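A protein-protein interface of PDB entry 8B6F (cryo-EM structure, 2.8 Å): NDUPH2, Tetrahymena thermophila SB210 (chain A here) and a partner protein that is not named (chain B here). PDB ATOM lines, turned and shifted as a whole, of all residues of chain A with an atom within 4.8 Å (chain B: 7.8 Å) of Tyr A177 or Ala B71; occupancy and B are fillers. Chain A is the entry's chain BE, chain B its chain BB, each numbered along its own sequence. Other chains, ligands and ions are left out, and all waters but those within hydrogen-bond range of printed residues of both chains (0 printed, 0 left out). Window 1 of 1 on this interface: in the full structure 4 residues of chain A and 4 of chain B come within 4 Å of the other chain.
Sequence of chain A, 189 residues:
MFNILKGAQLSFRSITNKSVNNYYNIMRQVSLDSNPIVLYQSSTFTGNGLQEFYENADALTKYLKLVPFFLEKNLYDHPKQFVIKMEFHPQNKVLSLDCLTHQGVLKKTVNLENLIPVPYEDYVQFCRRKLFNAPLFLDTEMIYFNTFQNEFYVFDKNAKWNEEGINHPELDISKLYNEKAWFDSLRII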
ATOM      1  N   ILE A 173      -1.785 -20.390  16.090  1.00  0.00           N
ATOM      2  CA  ILE A 173      -2.649 -20.236  17.257  1.00  0.00           C
ATOM      3  C   ILE A 173      -4.060 -19.862  16.829  1.00  0.00           C
ATOM      4  O   ILE A 173      -5.033 -20.192  17.514  1.00  0.00           O
ATOM      5  CB  ILE A 173      -2.065 -19.202  18.240  1.00  0.00           C
ATOM      6  CG1 ILE A 173      -2.045 -17.806  17.609  1.00  0.00           C
ATOM      7  CG2 ILE A 173      -0.672 -19.632  18.683  1.00  0.00           C
ATOM      8  CD1 ILE A 173      -1.526 -16.722  18.533  1.00  0.00           C
ATOM      9  N   SER A 174      -4.201 -19.182  15.689  1.00  0.00           N
ATOM     10  CA  SER A 174      -5.527 -18.810  15.213  1.00  0.00           C
ATOM     11  C   SER A 174      -6.413 -20.026  14.991  1.00  0.00           C
ATOM     12  O   SER A 174      -7.641 -19.892  14.981  1.00  0.00           O
ATOM     13  CB  SER A 174      -5.418 -18.012  13.913  1.00  0.00           C
ATOM     14  OG  SER A 174      -4.579 -16.881  14.076  1.00  0.00           O
ATOM     15  N   LYS A 175      -5.821 -21.204  14.813  1.00  0.00           N
ATOM     16  CA  LYS A 175      -6.570 -22.442  14.655  1.00  0.00           C
ATOM     17  C   LYS A 175      -6.458 -23.377  15.849  1.00  0.00           C
ATOM     18  O   LYS A 175      -7.387 -24.149  16.095  1.00  0.00           O
ATOM     19  CB  LYS A 175      -6.096 -23.184  13.398  1.00  0.00           C
ATOM     20  CG  LYS A 175      -6.941 -24.389  13.033  1.00  0.00           C
ATOM     21  CD  LYS A 175      -6.493 -24.994  11.714  1.00  0.00           C
ATOM     22  CE  LYS A 175      -7.367 -26.179  11.330  1.00  0.00           C
ATOM     23  NZ  LYS A 175      -6.977 -26.754  10.012  1.00  0.00           N
ATOM     24  N   LEU A 176      -5.356 -23.329  16.596  1.00  0.00           N
ATOM     25  CA  LEU A 176      -5.129 -24.227  17.720  1.00  0.00           C
ATOM     26  C   LEU A 176      -5.445 -23.594  19.069  1.00  0.00           C
ATOM     27  O   LEU A 176      -5.175 -24.209  20.105  1.00  0.00           O
ATOM     28  CB  LEU A 176      -3.678 -24.715  17.714  1.00  0.00           C
ATOM     29  CG  LEU A 176      -3.235 -25.540  16.505  1.00  0.00           C
ATOM     30  CD1 LEU A 176      -1.792 -25.981  16.674  1.00  0.00           C
ATOM     31  CD2 LEU A 176      -4.137 -26.745  16.289  1.00  0.00           C
ATOM     32  N   TYR A 177      -6.014 -22.393  19.090  1.00  0.00           N
ATOM     33  CA  TYR A 177      -6.245 -21.680  20.338  1.00  0.00           C
ATOM     34  C   TYR A 177      -7.627 -21.995  20.893  1.00  0.00           C
ATOM     35  O   TYR A 177      -8.620 -22.005  20.161  1.00  0.00           O
ATOM     36  CB  TYR A 177      -6.104 -20.170  20.131  1.00  0.00           C
ATOM     37  CG  TYR A 177      -6.446 -19.349  21.352  1.00  0.00           C
ATOM     38  CD1 TYR A 177      -5.490 -19.067  22.318  1.00  0.00           C
ATOM     39  CD2 TYR A 177      -7.726 -18.843  21.531  1.00  0.00           C
ATOM     40  CE1 TYR A 177      -5.804 -18.310  23.432  1.00  0.00           C
ATOM     41  CE2 TYR A 177      -8.048 -18.087  22.638  1.00  0.00           C
ATOM     42  CZ  TYR A 177      -7.084 -17.824  23.585  1.00  0.00           C
ATOM     43  OH  TYR A 177      -7.406 -17.071  24.688  1.00  0.00           O
ATOM     44  N   ASN A 178      -7.676 -22.250  22.198  1.00  0.00           N
ATOM     45  CA  ASN A 178      -8.938 -22.468  22.898  1.00  0.00           C
ATOM     46  C   ASN A 178      -8.761 -21.922  24.307  1.00  0.00           C
ATOM     47  O   ASN A 178      -7.967 -22.460  25.083  1.00  0.00           O
ATOM     48  CB  ASN A 178      -9.313 -23.947  22.915  1.00  0.00           C
ATOM     49  CG  ASN A 178     -10.651 -24.200  23.574  1.00  0.00           C
ATOM     50  OD1 ASN A 178     -10.720 -24.534  24.756  1.00  0.00           O
ATOM     51  ND2 ASN A 178     -11.727 -24.040  22.811  1.00  0.00           N
ATOM     52  N   GLU A 179      -9.494 -20.856  24.633  1.00  0.00           N
ATOM     53  CA  GLU A 179      -9.300 -20.197  25.921  1.00  0.00           C
ATOM     54  C   GLU A 179      -9.593 -21.145  27.074  1.00  0.00           C
ATOM     55  O   GLU A 179      -8.803 -21.256  28.018  1.00  0.00           O
ATOM     56  CB  GLU A 179     -10.186 -18.954  26.008  1.00  0.00           C
ATOM     57  CG  GLU A 179     -10.015 -18.170  27.298  1.00  0.00           C
ATOM     58  CD  GLU A 179     -10.931 -16.968  27.371  1.00  0.00           C
ATOM     59  OE1 GLU A 179     -11.676 -16.729  26.398  1.00  0.00           O
ATOM     60  OE2 GLU A 179     -10.905 -16.261  28.399  1.00  0.00           O
ATOM     61  N   TRP A 182      -6.806 -23.899  27.273  1.00  0.00           N
ATOM     62  CA  TRP A 182      -5.450 -23.454  27.580  1.00  0.00           C
ATOM     63  C   TRP A 182      -5.354 -22.852  28.976  1.00  0.00           C
ATOM     64  O   TRP A 182      -4.353 -23.051  29.672  1.00  0.00           O
ATOM     65  CB  TRP A 182      -4.976 -22.446  26.533  1.00  0.00           C
ATOM     66  CG  TRP A 182      -4.576 -23.077  25.234  1.00  0.00           C
ATOM     67  CD1 TRP A 182      -4.898 -24.327  24.797  1.00  0.00           C
ATOM     68  CD2 TRP A 182      -3.767 -22.489  24.209  1.00  0.00           C
ATOM     69  NE1 TRP A 182      -4.343 -24.554  23.562  1.00  0.00           N
ATOM     70  CE2 TRP A 182      -3.645 -23.441  23.177  1.00  0.00           C
ATOM     71  CE3 TRP A 182      -3.137 -21.249  24.063  1.00  0.00           C
ATOM     72  CZ2 TRP A 182      -2.919 -23.192  22.015  1.00  0.00           C
ATOM     73  CZ3 TRP A 182      -2.416 -21.002  22.907  1.00  0.00           C
ATOM     74  CH2 TRP A 182      -2.314 -21.969  21.898  1.00  0.00           C
ATOM     75  N   PHE A 183      -6.379 -22.118  29.406  1.00  0.00           N
ATOM     76  CA  PHE A 183      -6.315 -21.376  30.658  1.00  0.00           C
ATOM     77  C   PHE A 183      -6.997 -22.074  31.826  1.00  0.00           C
ATOM     78  O   PHE A 183      -6.598 -21.854  32.974  1.00  0.00           O
ATOM     79  CB  PHE A 183      -6.944 -19.991  30.481  1.00  0.00           C
ATOM     80  CG  PHE A 183      -6.148 -19.074  29.600  1.00  0.00           C
ATOM     81  CD1 PHE A 183      -5.166 -18.259  30.137  1.00  0.00           C
ATOM     82  CD2 PHE A 183      -6.384 -19.024  28.236  1.00  0.00           C
ATOM     83  CE1 PHE A 183      -4.431 -17.412  29.329  1.00  0.00           C
ATOM     84  CE2 PHE A 183      -5.653 -18.179  27.423  1.00  0.00           C
ATOM     85  CZ  PHE A 183      -4.676 -17.373  27.970  1.00  0.00           C
ATOM     86  N   PHE B  65     -12.891  -8.896  22.775  1.00  0.00           N
ATOM     87  CA  PHE B  65     -12.093  -9.740  23.657  1.00  0.00           C
ATOM     88  C   PHE B  65     -11.657 -11.033  22.980  1.00  0.00           C
ATOM     89  O   PHE B  65     -10.561 -11.528  23.258  1.00  0.00           O
ATOM     90  CB  PHE B  65     -12.877 -10.063  24.930  1.00  0.00           C
ATOM     91  CG  PHE B  65     -12.070 -10.785  25.971  1.00  0.00           C
ATOM     92  CD1 PHE B  65     -11.945 -12.164  25.941  1.00  0.00           C
ATOM     93  CD2 PHE B  65     -11.437 -10.083  26.982  1.00  0.00           C
ATOM     94  CE1 PHE B  65     -11.202 -12.827  26.898  1.00  0.00           C
ATOM     95  CE2 PHE B  65     -10.693 -10.740  27.941  1.00  0.00           C
ATOM     96  CZ  PHE B  65     -10.576 -12.112  27.901  1.00  0.00           C
ATOM     97  N   LYS B  66     -12.493 -11.599  22.108  1.00  0.00           N
ATOM     98  CA  LYS B  66     -12.163 -12.880  21.491  1.00  0.00           C
ATOM     99  C   LYS B  66     -11.165 -12.708  20.352  1.00  0.00           C
ATOM    100  O   LYS B  66     -10.137 -13.392  20.312  1.00  0.00           O
ATOM    101  CB  LYS B  66     -13.436 -13.562  20.985  1.00  0.00           C
ATOM    102  CG  LYS B  66     -14.255 -14.261  22.064  1.00  0.00           C
ATOM    103  CD  LYS B  66     -14.818 -13.277  23.079  1.00  0.00           C
ATOM    104  CE  LYS B  66     -15.806 -13.956  24.017  1.00  0.00           C
ATOM    105  NZ  LYS B  66     -16.302 -13.026  25.072  1.00  0.00           N
ATOM    106  N   ASP B  67     -11.449 -11.798  19.417  1.00  0.00           N
ATOM    107  CA  ASP B  67     -10.579 -11.640  18.255  1.00  0.00           C
ATOM    108  C   ASP B  67      -9.174 -11.226  18.672  1.00  0.00           C
ATOM    109  O   ASP B  67      -8.184 -11.744  18.142  1.00  0.00           O
ATOM    110  CB  ASP B  67     -11.176 -10.623  17.285  1.00  0.00           C
ATOM    111  CG  ASP B  67     -12.611 -10.944  16.919  1.00  0.00           C
ATOM    112  OD1 ASP B  67     -12.980 -12.135  16.953  1.00  0.00           O
ATOM    113  OD2 ASP B  67     -13.371 -10.005  16.603  1.00  0.00           O
ATOM    114  N   ASP B  68      -9.065 -10.293  19.611  1.00  0.00           N
ATOM    115  CA  ASP B  68      -7.780  -9.912  20.178  1.00  0.00           C
ATOM    116  C   ASP B  68      -7.488 -10.806  21.373  1.00  0.00           C
ATOM    117  O   ASP B  68      -8.356 -11.012  22.227  1.00  0.00           O
ATOM    118  CB  ASP B  68      -7.788  -8.446  20.610  1.00  0.00           C
ATOM    119  CG  ASP B  68      -8.367  -7.529  19.556  1.00  0.00           C
ATOM    120  OD1 ASP B  68      -8.288  -7.875  18.359  1.00  0.00           O
ATOM    121  OD2 ASP B  68      -8.907  -6.466  19.923  1.00  0.00           O
ATOM    122  N   LEU B  69      -6.269 -11.333  21.438  1.00  0.00           N
ATOM    123  CA  LEU B  69      -5.913 -12.235  22.522  1.00  0.00           C
ATOM    124  C   LEU B  69      -5.726 -11.451  23.813  1.00  0.00           C
ATOM    125  O   LEU B  69      -4.614 -11.359  24.341  1.00  0.00           O
ATOM    126  CB  LEU B  69      -4.647 -13.019  22.174  1.00  0.00           C
ATOM    127  CG  LEU B  69      -4.752 -13.934  20.952  1.00  0.00           C
ATOM    128  CD1 LEU B  69      -3.432 -14.636  20.705  1.00  0.00           C
ATOM    129  CD2 LEU B  69      -5.870 -14.954  21.111  1.00  0.00           C
ATOM    130  N   VAL B  70      -6.819 -10.885  24.325  1.00  0.00           N
ATOM    131  CA  VAL B  70      -6.749 -10.112  25.560  1.00  0.00           C
ATOM    132  C   VAL B  70      -6.288 -10.993  26.710  1.00  0.00           C
ATOM    133  O   VAL B  70      -5.515 -10.560  27.573  1.00  0.00           O
ATOM    134  CB  VAL B  70      -8.114  -9.461  25.855  1.00  0.00           C
ATOM    135  CG1 VAL B  70      -8.117  -8.806  27.226  1.00  0.00           C
ATOM    136  CG2 VAL B  70      -8.461  -8.447  24.778  1.00  0.00           C
ATOM    137  N   ALA B  71      -6.752 -12.242  26.743  1.00  0.00           N
ATOM    138  CA  ALA B  71      -6.358 -13.147  27.814  1.00  0.00           C
ATOM    139  C   ALA B  71      -4.852 -13.359  27.859  1.00  0.00           C
ATOM    140  O   ALA B  71      -4.325 -13.756  28.904  1.00  0.00           O
ATOM    141  CB  ALA B  71      -7.068 -14.490  27.651  1.00  0.00           C
ATOM    142  N   VAL B  72      -4.152 -13.108  26.758  1.00  0.00           N
ATOM    143  CA  VAL B  72      -2.705 -13.246  26.706  1.00  0.00           C
ATOM    144  C   VAL B  72      -2.008 -11.897  26.818  1.00  0.00           C
ATOM    145  O   VAL B  72      -1.034 -11.762  27.558  1.00  0.00           O
ATOM    146  CB  VAL B  72      -2.289 -13.979  25.410  1.00  0.00           C
ATOM    147  CG1 VAL B  72      -0.783 -14.191  25.374  1.00  0.00           C
ATOM    148  CG2 VAL B  72      -3.018 -15.308  25.292  1.00  0.00           C
ATOM    149  N   TYR B  73      -2.494 -10.889  26.093  1.00  0.00           N
ATOM    150  CA  TYR B  73      -1.847  -9.584  26.048  1.00  0.00           C
ATOM    151  C   TYR B  73      -2.569  -8.520  26.862  1.00  0.00           C
ATOM    152  O   TYR B  73      -2.060  -7.398  26.969  1.00  0.00           O
ATOM    153  CB  TYR B  73      -1.732  -9.110  24.596  1.00  0.00           C
ATOM    154  CG  TYR B  73      -1.015 -10.087  23.696  1.00  0.00           C
ATOM    155  CD1 TYR B  73       0.368 -10.073  23.584  1.00  0.00           C
ATOM    156  CD2 TYR B  73      -1.722 -11.025  22.961  1.00  0.00           C
ATOM    157  CE1 TYR B  73       1.027 -10.966  22.763  1.00  0.00           C
ATOM    158  CE2 TYR B  73      -1.074 -11.923  22.138  1.00  0.00           C
ATOM    159  CZ  TYR B  73       0.300 -11.888  22.043  1.00  0.00           C
ATOM    160  OH  TYR B  73       0.950 -12.781  21.223  1.00  0.00           O
ATOM    161  N   GLY B  74      -3.728  -8.828  27.429  1.00  0.00           N
ATOM    162  CA  GLY B  74      -4.439  -7.854  28.229  1.00  0.00           C
ATOM    163  C   GLY B  74      -5.113  -6.788  27.378  1.00  0.00           C
ATOM    164  O   GLY B  74      -5.217  -6.883  26.156  1.00  0.00           O
ATOM    165  N   PHE B  75      -5.578  -5.750  28.067  1.00  0.00           N
ATOM    166  CA  PHE B  75      -6.283  -4.641  27.442  1.00  0.00           C
ATOM    167  C   PHE B  75      -5.322  -3.495  27.162  1.00  0.00           C
ATOM    168  O   PHE B  75      -4.457  -3.181  27.983  1.00  0.00           O
ATOM    169  CB  PHE B  75      -7.418  -4.140  28.338  1.00  0.00           C
ATOM    170  CG  PHE B  75      -8.557  -5.105  28.478  1.00  0.00           C
ATOM    171  CD1 PHE B  75      -9.537  -5.185  27.504  1.00  0.00           C
ATOM    172  CD2 PHE B  75      -8.663  -5.910  29.598  1.00  0.00           C
ATOM    173  CE1 PHE B  75     -10.593  -6.065  27.636  1.00  0.00           C
ATOM    174  CE2 PHE B  75      -9.717  -6.793  29.737  1.00  0.00           C
ATOM    175  CZ  PHE B  75     -10.684  -6.869  28.755  1.00  0.00           C
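Of the 9 printed residues of chain A, 4 touch a printed residue of chain B.
Printed residues of chain A that touch a printed residue of chain B: Ile A173, Tyr A177, Glu A179 and Phe A183.
Hydrophobic or aromatic side chains of chain A within 4 Å of the printed part of chain B: Ile A173, Tyr A177 and Phe A183.
Of the 11 printed residues of chain B, 4 touch a printed residue of chain A.
Printed residues of chain B that touch a printed residue of chain A: Phe B65, Leu B69, Ala B71 and Val B72.
Hydrophobic or aromatic side chains of chain B that line the printed part of chain A: Phe B65, Leu B69, Ala B71 and Val B72.
Along chain B the printed residues that touch a printed residue of chain A span positions 65 to 72.
Among the printed residues, 6 pairs touch across the chains.
Among the printed residues, no Asp or Glu carboxylate lies within 4 Å of a Lys or Arg side-chain nitrogen of the other chain.
Ile A173 touches Leu B69.
Leu B69 touches Tyr A177.
Tyr A177 touches Ala B71 (OH to CB, 3.9 Å).
Glu A179 touches Phe B65.
Ala B71 touches Phe A183.
Phe A183 touches Val B72 (CZ to CG2, 3.8 Å).
Tyr A177 touches two residues of chain B.
Of the printed residues of chain A, Ala B71 touches Tyr A177 (3.9 Å) and Phe A183 (3.7 Å).
Of the printed residues of chain B, Phe A183 touches Ala B71 and Val B72.
Printed residues of chain B within 4 Å of Glu A179: Phe B65 (3.8 Å).
Of the printed residues of chain B, Ile A173 touches Leu B69.
The nearest residue of chain B that does not touch Tyr A177 is Val B72 (4.5 Å).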
